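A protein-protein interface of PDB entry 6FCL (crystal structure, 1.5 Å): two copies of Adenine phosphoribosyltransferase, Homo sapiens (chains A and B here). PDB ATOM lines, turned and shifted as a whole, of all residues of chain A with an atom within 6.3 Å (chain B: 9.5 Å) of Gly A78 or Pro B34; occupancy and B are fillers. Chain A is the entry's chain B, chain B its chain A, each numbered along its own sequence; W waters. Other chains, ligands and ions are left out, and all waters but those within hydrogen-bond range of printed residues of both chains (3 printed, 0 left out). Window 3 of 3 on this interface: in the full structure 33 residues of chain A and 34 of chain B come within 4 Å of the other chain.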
ATOM      1  N   TYR A  58     -21.360 -23.477 -15.483  1.00  0.00           N
ATOM      2  CA  TYR A  58     -21.454 -22.835 -14.166  1.00  0.00           C
ATOM      3  C   TYR A  58     -20.615 -23.555 -13.126  1.00  0.00           C
ATOM      4  O   TYR A  58     -20.396 -24.767 -13.216  1.00  0.00           O
ATOM      5  CB  TYR A  58     -22.914 -22.814 -13.666  1.00  0.00           C
ATOM      6  CG  TYR A  58     -23.823 -21.912 -14.462  1.00  0.00           C
ATOM      7  CD1 TYR A  58     -23.773 -20.537 -14.301  1.00  0.00           C
ATOM      8  CD2 TYR A  58     -24.682 -22.424 -15.421  1.00  0.00           C
ATOM      9  CE1 TYR A  58     -24.559 -19.691 -15.058  1.00  0.00           C
ATOM     10  CE2 TYR A  58     -25.494 -21.582 -16.166  1.00  0.00           C
ATOM     11  CZ  TYR A  58     -25.419 -20.215 -15.982  1.00  0.00           C
ATOM     12  OH  TYR A  58     -26.221 -19.371 -16.739  1.00  0.00           O
ATOM     13  N   LEU A  73     -13.628 -18.656  -8.066  1.00  0.00           N
ATOM     14  CA  LEU A  73     -13.306 -19.662  -9.088  1.00  0.00           C
ATOM     15  C   LEU A  73     -14.107 -19.410 -10.362  1.00  0.00           C
ATOM     16  O   LEU A  73     -13.570 -19.434 -11.469  1.00  0.00           O
ATOM     17  CB  LEU A  73     -13.561 -21.070  -8.554  1.00  0.00           C
ATOM     18  CG  LEU A  73     -13.310 -22.222  -9.538  1.00  0.00           C
ATOM     19  CD1 LEU A  73     -11.913 -22.211 -10.132  1.00  0.00           C
ATOM     20  CD2 LEU A  73     -13.596 -23.555  -8.859  1.00  0.00           C
ATOM     21  N   ALA A  74     -15.407 -19.185 -10.205  1.00  0.00           N
ATOM     22  CA  ALA A  74     -16.249 -18.828 -11.337  1.00  0.00           C
ATOM     23  C   ALA A  74     -15.715 -17.600 -12.081  1.00  0.00           C
ATOM     24  O   ALA A  74     -15.559 -17.629 -13.302  1.00  0.00           O
ATOM     25  CB  ALA A  74     -17.674 -18.586 -10.859  1.00  0.00           C
ATOM     26  N   GLN A  75     -15.431 -16.531 -11.349  1.00  0.00           N
ATOM     27  CA  GLN A  75     -14.881 -15.325 -11.962  1.00  0.00           C
ATOM     28  C   GLN A  75     -13.597 -15.594 -12.745  1.00  0.00           C
ATOM     29  O   GLN A  75     -13.420 -15.096 -13.869  1.00  0.00           O
ATOM     30  CB  GLN A  75     -14.637 -14.262 -10.900  1.00  0.00           C
ATOM     31  CG  GLN A  75     -15.875 -13.464 -10.540  1.00  0.00           C
ATOM     32  CD  GLN A  75     -16.276 -12.464 -11.616  1.00  0.00           C
ATOM     33  OE1 GLN A  75     -15.550 -11.516 -11.907  1.00  0.00           O
ATOM     34  NE2 GLN A  75     -17.455 -12.653 -12.181  1.00  0.00           N
ATOM     35  N   GLU A  76     -12.688 -16.360 -12.156  1.00  0.00           N
ATOM     36  CA  GLU A  76     -11.420 -16.667 -12.823  1.00  0.00           C
ATOM     37  C   GLU A  76     -11.666 -17.394 -14.155  1.00  0.00           C
ATOM     38  O   GLU A  76     -10.905 -17.231 -15.116  1.00  0.00           O
ATOM     39  CB  GLU A  76     -10.528 -17.506 -11.908  1.00  0.00           C
ATOM     40  CG  GLU A  76      -9.186 -17.901 -12.511  1.00  0.00           C
ATOM     41  CD  GLU A  76      -8.288 -16.716 -12.832  1.00  0.00           C
ATOM     42  OE1 GLU A  76      -8.501 -15.622 -12.274  1.00  0.00           O
ATOM     43  OE2 GLU A  76      -7.348 -16.891 -13.640  1.00  0.00           O
ATOM     44  N   LEU A  77     -12.746 -18.164 -14.218  1.00  0.00           N
ATOM     45  CA  LEU A  77     -13.085 -18.938 -15.405  1.00  0.00           C
ATOM     46  C   LEU A  77     -14.027 -18.213 -16.370  1.00  0.00           C
ATOM     47  O   LEU A  77     -14.364 -18.752 -17.428  1.00  0.00           O
ATOM     48  CB  LEU A  77     -13.728 -20.266 -14.990  1.00  0.00           C
ATOM     49  CG  LEU A  77     -12.831 -21.293 -14.305  1.00  0.00           C
ATOM     50  CD1 LEU A  77     -13.675 -22.388 -13.682  1.00  0.00           C
ATOM     51  CD2 LEU A  77     -11.857 -21.882 -15.308  1.00  0.00           C
ATOM     52  N   GLY A  78     -14.506 -17.038 -15.964  1.00  0.00           N
ATOM     53  CA  GLY A  78     -15.445 -16.263 -16.766  1.00  0.00           C
ATOM     54  C   GLY A  78     -16.880 -16.774 -16.703  1.00  0.00           C
ATOM     55  O   GLY A  78     -17.667 -16.536 -17.615  1.00  0.00           O
ATOM     56  N   LEU A  79     -17.219 -17.450 -15.615  1.00  0.00           N
ATOM     57  CA  LEU A  79     -18.509 -18.125 -15.460  1.00  0.00           C
ATOM     58  C   LEU A  79     -19.284 -17.574 -14.282  1.00  0.00           C
ATOM     59  O   LEU A  79     -18.703 -16.960 -13.397  1.00  0.00           O
ATOM     60  CB  LEU A  79     -18.286 -19.606 -15.186  1.00  0.00           C
ATOM     61  CG  LEU A  79     -17.438 -20.352 -16.212  1.00  0.00           C
ATOM     62  CD1 LEU A  79     -17.250 -21.795 -15.768  1.00  0.00           C
ATOM     63  CD2 LEU A  79     -18.065 -20.277 -17.587  1.00  0.00           C
ATOM     64  N   GLY A  80     -20.587 -17.839 -14.266  1.00  0.00           N
ATOM     65  CA  GLY A  80     -21.414 -17.541 -13.111  1.00  0.00           C
ATOM     66  C   GLY A  80     -21.334 -18.673 -12.098  1.00  0.00           C
ATOM     67  O   GLY A  80     -20.810 -19.754 -12.387  1.00  0.00           O
ATOM     68  N   CYS A  81     -21.772 -18.368 -10.884  1.00  0.00           N
ATOM     69  CA  CYS A  81     -21.803 -19.315  -9.787  1.00  0.00           C
ATOM     70  C   CYS A  81     -23.235 -19.491  -9.308  1.00  0.00           C
ATOM     71  O   CYS A  81     -23.938 -18.499  -9.099  1.00  0.00           O
ATOM     72  CB  CYS A  81     -20.940 -18.777  -8.646  1.00  0.00           C
ATOM     73  SG  CYS A  81     -20.716 -19.925  -7.287  1.00  0.00           S
ATOM     74  N   GLU B   3     -22.864   0.278 -14.459  1.00  0.00           N
ATOM     75  CA  GLU B   3     -22.400  -0.809 -13.601  1.00  0.00           C
ATOM     76  C   GLU B   3     -23.398  -1.090 -12.487  1.00  0.00           C
ATOM     77  O   GLU B   3     -23.720  -2.250 -12.208  1.00  0.00           O
ATOM     78  CB  GLU B   3     -21.029  -0.492 -12.996  1.00  0.00           C
ATOM     79  CG  GLU B   3     -19.898  -1.315 -13.585  1.00  0.00           C
ATOM     80  CD  GLU B   3     -19.669  -1.027 -15.050  1.00  0.00           C
ATOM     81  OE1 GLU B   3     -19.693  -1.981 -15.856  1.00  0.00           O
ATOM     82  OE2 GLU B   3     -19.484   0.158 -15.397  1.00  0.00           O
ATOM     83  N   LEU B   6     -26.293  -2.990 -13.771  1.00  0.00           N
ATOM     84  CA  LEU B   6     -26.002  -4.414 -13.943  1.00  0.00           C
ATOM     85  C   LEU B   6     -26.261  -5.197 -12.646  1.00  0.00           C
ATOM     86  O   LEU B   6     -26.608  -6.383 -12.683  1.00  0.00           O
ATOM     87  CB  LEU B   6     -24.548  -4.629 -14.372  1.00  0.00           C
ATOM     88  CG  LEU B   6     -24.094  -4.190 -15.768  1.00  0.00           C
ATOM     89  CD1 LEU B   6     -22.608  -4.486 -15.918  1.00  0.00           C
ATOM     90  CD2 LEU B   6     -24.884  -4.893 -16.861  1.00  0.00           C
ATOM     91  N   VAL B   7     -26.067  -4.551 -11.502  1.00  0.00           N
ATOM     92  CA  VAL B   7     -26.349  -5.191 -10.218  1.00  0.00           C
ATOM     93  C   VAL B   7     -27.847  -5.131  -9.898  1.00  0.00           C
ATOM     94  O   VAL B   7     -28.455  -6.135  -9.524  1.00  0.00           O
ATOM     95  CB  VAL B   7     -25.528  -4.540  -9.076  1.00  0.00           C
ATOM     96  CG1 VAL B   7     -25.765  -5.240  -7.742  1.00  0.00           C
ATOM     97  CG2 VAL B   7     -24.049  -4.531  -9.421  1.00  0.00           C
ATOM     98  N   ARG B  10     -30.271  -7.520 -11.417  1.00  0.00           N
ATOM     99  CA  ARG B  10     -30.077  -8.916 -11.029  1.00  0.00           C
ATOM    100  C   ARG B  10     -30.462  -9.184  -9.573  1.00  0.00           C
ATOM    101  O   ARG B  10     -30.050 -10.193  -8.989  1.00  0.00           O
ATOM    102  CB  ARG B  10     -28.620  -9.319 -11.255  1.00  0.00           C
ATOM    103  CG  ARG B  10     -28.192  -9.336 -12.714  1.00  0.00           C
ATOM    104  CD  ARG B  10     -28.868 -10.442 -13.501  1.00  0.00           C
ATOM    105  NE  ARG B  10     -28.456 -10.418 -14.900  1.00  0.00           N
ATOM    106  CZ  ARG B  10     -29.013 -11.149 -15.857  1.00  0.00           C
ATOM    107  NH1 ARG B  10     -30.023 -11.958 -15.575  1.00  0.00           N
ATOM    108  NH2 ARG B  10     -28.566 -11.059 -17.099  1.00  0.00           N
ATOM    109  N   SER B  28     -28.959 -14.005  -5.629  1.00  0.00           N
ATOM    110  CA  SER B  28     -28.466 -15.147  -6.406  1.00  0.00           C
ATOM    111  C   SER B  28     -28.189 -14.803  -7.870  1.00  0.00           C
ATOM    112  O   SER B  28     -27.168 -15.194  -8.426  1.00  0.00           O
ATOM    113  CB  SER B  28     -29.454 -16.309  -6.320  1.00  0.00           C
ATOM    114  OG  SER B  28     -29.483 -16.827  -5.000  1.00  0.00           O
ATOM    115  N   PRO B  29     -29.087 -14.038  -8.501  1.00  0.00           N
ATOM    116  CA  PRO B  29     -28.810 -13.760  -9.912  1.00  0.00           C
ATOM    117  C   PRO B  29     -27.552 -12.915 -10.163  1.00  0.00           C
ATOM    118  O   PRO B  29     -27.000 -12.951 -11.254  1.00  0.00           O
ATOM    119  CB  PRO B  29     -30.078 -13.027 -10.382  1.00  0.00           C
ATOM    120  CG  PRO B  29     -31.143 -13.468  -9.421  1.00  0.00           C
ATOM    121  CD  PRO B  29     -30.433 -13.581  -8.104  1.00  0.00           C
ATOM    122  N   VAL B  30     -27.132 -12.142  -9.176  1.00  0.00           N
ATOM    123  CA  VAL B  30     -25.900 -11.369  -9.265  1.00  0.00           C
ATOM    124  C   VAL B  30     -24.722 -12.333  -9.365  1.00  0.00           C
ATOM    125  O   VAL B  30     -23.794 -12.116 -10.134  1.00  0.00           O
ATOM    126  CB  VAL B  30     -25.699 -10.460  -8.020  1.00  0.00           C
ATOM    127  CG1 VAL B  30     -24.347  -9.771  -8.059  1.00  0.00           C
ATOM    128  CG2 VAL B  30     -26.819  -9.430  -7.909  1.00  0.00           C
ATOM    129  N   LEU B  31     -24.757 -13.393  -8.564  1.00  0.00           N
ATOM    130  CA  LEU B  31     -23.688 -14.393  -8.590  1.00  0.00           C
ATOM    131  C   LEU B  31     -23.689 -15.178  -9.901  1.00  0.00           C
ATOM    132  O   LEU B  31     -22.643 -15.597 -10.373  1.00  0.00           O
ATOM    133  CB  LEU B  31     -23.841 -15.372  -7.426  1.00  0.00           C
ATOM    134  CG  LEU B  31     -23.250 -14.953  -6.075  1.00  0.00           C
ATOM    135  CD1 LEU B  31     -21.729 -15.048  -6.093  1.00  0.00           C
ATOM    136  CD2 LEU B  31     -23.690 -13.564  -5.668  1.00  0.00           C
ATOM    137  N   LYS B  32     -24.873 -15.401 -10.465  1.00  0.00           N
ATOM    138  CA  LYS B  32     -25.013 -16.257 -11.648  1.00  0.00           C
ATOM    139  C   LYS B  32     -24.567 -15.579 -12.945  1.00  0.00           C
ATOM    140  O   LYS B  32     -24.227 -16.244 -13.930  1.00  0.00           O
ATOM    141  CB  LYS B  32     -26.464 -16.704 -11.785  1.00  0.00           C
ATOM    142  CG  LYS B  32     -26.656 -17.759 -12.857  1.00  0.00           C
ATOM    143  CD  LYS B  32     -28.078 -18.274 -12.883  1.00  0.00           C
ATOM    144  CE  LYS B  32     -28.227 -19.411 -13.872  1.00  0.00           C
ATOM    145  NZ  LYS B  32     -29.623 -19.915 -13.931  1.00  0.00           N
ATOM    146  N   ASP B  33     -24.614 -14.251 -12.951  1.00  0.00           N
ATOM    147  CA  ASP B  33     -24.223 -13.447 -14.102  1.00  0.00           C
ATOM    148  C   ASP B  33     -22.827 -12.881 -13.834  1.00  0.00           C
ATOM    149  O   ASP B  33     -22.663 -11.982 -13.004  1.00  0.00           O
ATOM    150  CB  ASP B  33     -25.265 -12.333 -14.303  1.00  0.00           C
ATOM    151  CG  ASP B  33     -24.931 -11.397 -15.448  1.00  0.00           C
ATOM    152  OD1 ASP B  33     -23.828 -11.486 -16.024  1.00  0.00           O
ATOM    153  OD2 ASP B  33     -25.795 -10.541 -15.752  1.00  0.00           O
ATOM    154  N   PRO B  34     -21.800 -13.430 -14.502  1.00  0.00           N
ATOM    155  CA  PRO B  34     -20.450 -12.995 -14.165  1.00  0.00           C
ATOM    156  C   PRO B  34     -20.229 -11.480 -14.299  1.00  0.00           C
ATOM    157  O   PRO B  34     -19.423 -10.905 -13.556  1.00  0.00           O
ATOM    158  CB  PRO B  34     -19.562 -13.785 -15.131  1.00  0.00           C
ATOM    159  CG  PRO B  34     -20.460 -14.215 -16.233  1.00  0.00           C
ATOM    160  CD  PRO B  34     -21.811 -14.395 -15.615  1.00  0.00           C
ATOM    161  N   ALA B  35     -20.938 -10.835 -15.218  1.00  0.00           N
ATOM    162  CA  ALA B  35     -20.745  -9.392 -15.413  1.00  0.00           C
ATOM    163  C   ALA B  35     -21.330  -8.605 -14.245  1.00  0.00           C
ATOM    164  O   ALA B  35     -20.768  -7.590 -13.822  1.00  0.00           O
ATOM    165  CB  ALA B  35     -21.363  -8.932 -16.732  1.00  0.00           C
ATOM    166  N   SER B  36     -22.433  -9.105 -13.708  1.00  0.00           N
ATOM    167  CA  SER B  36     -23.090  -8.499 -12.563  1.00  0.00           C
ATOM    168  C   SER B  36     -22.232  -8.629 -11.303  1.00  0.00           C
ATOM    169  O   SER B  36     -22.033  -7.653 -10.566  1.00  0.00           O
ATOM    170  CB  SER B  36     -24.461  -9.151 -12.350  1.00  0.00           C
ATOM    171  OG  SER B  36     -25.230  -8.461 -11.368  1.00  0.00           O
ATOM    172  N   PHE B  37     -21.705  -9.826 -11.060  1.00  0.00           N
ATOM    173  CA  PHE B  37     -20.859 -10.049  -9.898  1.00  0.00           C
ATOM    174  C   PHE B  37     -19.622  -9.153  -9.983  1.00  0.00           C
ATOM    175  O   PHE B  37     -19.250  -8.509  -9.009  1.00  0.00           O
ATOM    176  CB  PHE B  37     -20.449 -11.527  -9.819  1.00  0.00           C
ATOM    177  CG  PHE B  37     -19.642 -11.865  -8.591  1.00  0.00           C
ATOM    178  CD1 PHE B  37     -20.248 -11.936  -7.352  1.00  0.00           C
ATOM    179  CD2 PHE B  37     -18.265 -12.022  -8.668  1.00  0.00           C
ATOM    180  CE1 PHE B  37     -19.495 -12.230  -6.217  1.00  0.00           C
ATOM    181  CE2 PHE B  37     -17.512 -12.297  -7.543  1.00  0.00           C
ATOM    182  CZ  PHE B  37     -18.135 -12.432  -6.319  1.00  0.00           C
ATOM    183  N   ARG B  38     -18.977  -9.111 -11.146  1.00  0.00           N
ATOM    184  CA  ARG B  38     -17.786  -8.288 -11.325  1.00  0.00           C
ATOM    185  C   ARG B  38     -18.093  -6.808 -11.067  1.00  0.00           C
ATOM    186  O   ARG B  38     -17.290  -6.095 -10.464  1.00  0.00           O
ATOM    187  CB  ARG B  38     -17.233  -8.475 -12.731  1.00  0.00           C
ATOM    188  CG  ARG B  38     -15.989  -7.656 -13.016  1.00  0.00           C
ATOM    189  CD  ARG B  38     -15.240  -8.169 -14.240  1.00  0.00           C
ATOM    190  NE  ARG B  38     -16.069  -8.150 -15.443  1.00  0.00           N
ATOM    191  CZ  ARG B  38     -16.651  -9.220 -15.981  1.00  0.00           C
ATOM    192  NH1 ARG B  38     -16.485 -10.421 -15.441  1.00  0.00           N
ATOM    193  NH2 ARG B  38     -17.397  -9.086 -17.072  1.00  0.00           N
ATOM    194  N   ALA B  39     -19.263  -6.360 -11.525  1.00  0.00           N
ATOM    195  CA  ALA B  39     -19.699  -4.986 -11.319  1.00  0.00           C
ATOM    196  C   ALA B  39     -19.889  -4.681  -9.830  1.00  0.00           C
ATOM    197  O   ALA B  39     -19.441  -3.644  -9.336  1.00  0.00           O
ATOM    198  CB  ALA B  39     -20.990  -4.733 -12.075  1.00  0.00           C
ATOM    199  N   ALA B  40     -20.539  -5.590  -9.111  1.00  0.00           N
ATOM    200  CA  ALA B  40     -20.771  -5.391  -7.688  1.00  0.00           C
ATOM    201  C   ALA B  40     -19.453  -5.274  -6.917  1.00  0.00           C
ATOM    202  O   ALA B  40     -19.289  -4.401  -6.058  1.00  0.00           O
ATOM    203  CB  ALA B  40     -21.614  -6.525  -7.124  1.00  0.00           C
ATOM    204  N   ILE B  41     -18.539  -6.204  -7.171  1.00  0.00           N
ATOM    205  CA  ILE B  41     -17.252  -6.194  -6.479  1.00  0.00           C
ATOM    206  C   ILE B  41     -16.489  -4.910  -6.832  1.00  0.00           C
ATOM    207  O   ILE B  41     -15.903  -4.256  -5.960  1.00  0.00           O
ATOM    208  CB  ILE B  41     -16.411  -7.439  -6.847  1.00  0.00           C
ATOM    209  CG1 ILE B  41     -17.078  -8.723  -6.322  1.00  0.00           C
ATOM    210  CG2 ILE B  41     -14.994  -7.315  -6.299  1.00  0.00           C
ATOM    211  CD1 ILE B  41     -17.252  -8.801  -4.822  1.00  0.00           C
ATOM    212  N   GLY B  42     -16.514  -4.538  -8.109  1.00  0.00           N
ATOM    213  CA  GLY B  42     -15.824  -3.331  -8.553  1.00  0.00           C
ATOM    214  C   GLY B  42     -16.349  -2.058  -7.907  1.00  0.00           C
ATOM    215  O   GLY B  42     -15.569  -1.166  -7.538  1.00  0.00           O
HETATM  216  O   HOH W   1     -26.380 -17.773  -8.053  1.00  0.00           O
HETATM  217  O   HOH W   2     -15.568 -12.968 -14.804  1.00  0.00           O
HETATM  218  O   HOH W   3     -24.574 -16.664 -16.602  1.00  0.00           O
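The backbone carbonyl oxygen (O) of Pro B34 is in hydrogen-bond range of the side-chain amide nitrogen (NE2) of Gln A75. The backbone carbonyl oxygen (O) of Leu B31 is in hydrogen-bond range of the backbone NH (N) of Cys A81, 2.9 Å away.
The backbone carbonyl oxygen (O) of Ala A74 lies within hydrogen-bond range of the backbone NH (N) of Leu A79 (2.9 Å). The backbone NH (N) of Phe B37 is in hydrogen-bond range of the backbone carbonyl oxygen (O) of Val B30 (3.2 Å).
Among the printed residues, pairs that only touch across the chains: Gly A80 with Lys B32 (3.2 Å), Gln A75 with Phe B37 (3.4 Å), Tyr A58 with Lys B32 (3.5 Å), Cys A81 with Lys B32 (3.5 Å), Gln A75 with Arg B38 (3.6 Å), Gly A80 with Leu B31 (3.6 Å), Leu A79 with Pro B34 (3.7 Å), Gly A78 with Pro B34 (3.9 Å) and Gly A80 with Pro B34 (3.9 Å).
Of the printed residues of chain B, Gly A78 touches Pro B34 (3.9 Å). Printed residues of chain B within 4 Å of Cys A81: Leu B31 (2.9 Å) and Lys B32 (3.5 Å). Printed residues of chain A within 4 Å of Lys B32: Tyr A58, Gly A80 and Cys A81. Of chain A, only Gln A75 (3.0 Å), Gly A78 (3.9 Å), Leu A79 (3.7 Å) and Gly A80 (3.9 Å) come within 4 Å of Pro B34. Printed residues of chain A within 4 Å of Phe B37: Gln A75. The nearest residue of chain B that does not touch Gly A78 is Arg B38 (6.1 Å). The nearest printed residue of chain A that does not touch Arg B38 is Gly A78 (6.1 Å).
Hydrophobic or aromatic side chains of chain A within 4 Å of the printed part of chain B: Tyr A58. Along chain A the printed residues that touch a printed residue of chain B span positions 58 to 81. Of the 19 printed residues of chain B, 5 touch a printed residue of chain A. Printed residues of chain B that touch a printed residue of chain A: Leu B31, Lys B32, Pro B34, Phe B37 and Arg B38. Among the printed residues, no Asp or Glu carboxylate lies within 4 Å of a Lys or Arg side-chain nitrogen of the other chain.
No position is printed for both chains. Of the 11 pairs that touch across the chains among the printed residues, none has its exchanged pair printed and touching as well.
Water W1 lies within hydrogen-bond range of O of Ser B28 (2.7 Å) and O of Cys A81 (2.8 Å). Water W3 bridges O of Lys B32 (2.7 Å) and OH of Tyr A58 (3.2 Å). Water W2 bridges the guanidinium group of Arg B38 (2.8 Å) and the backbone carbonyl oxygen of Gln A75 (3.2 Å).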
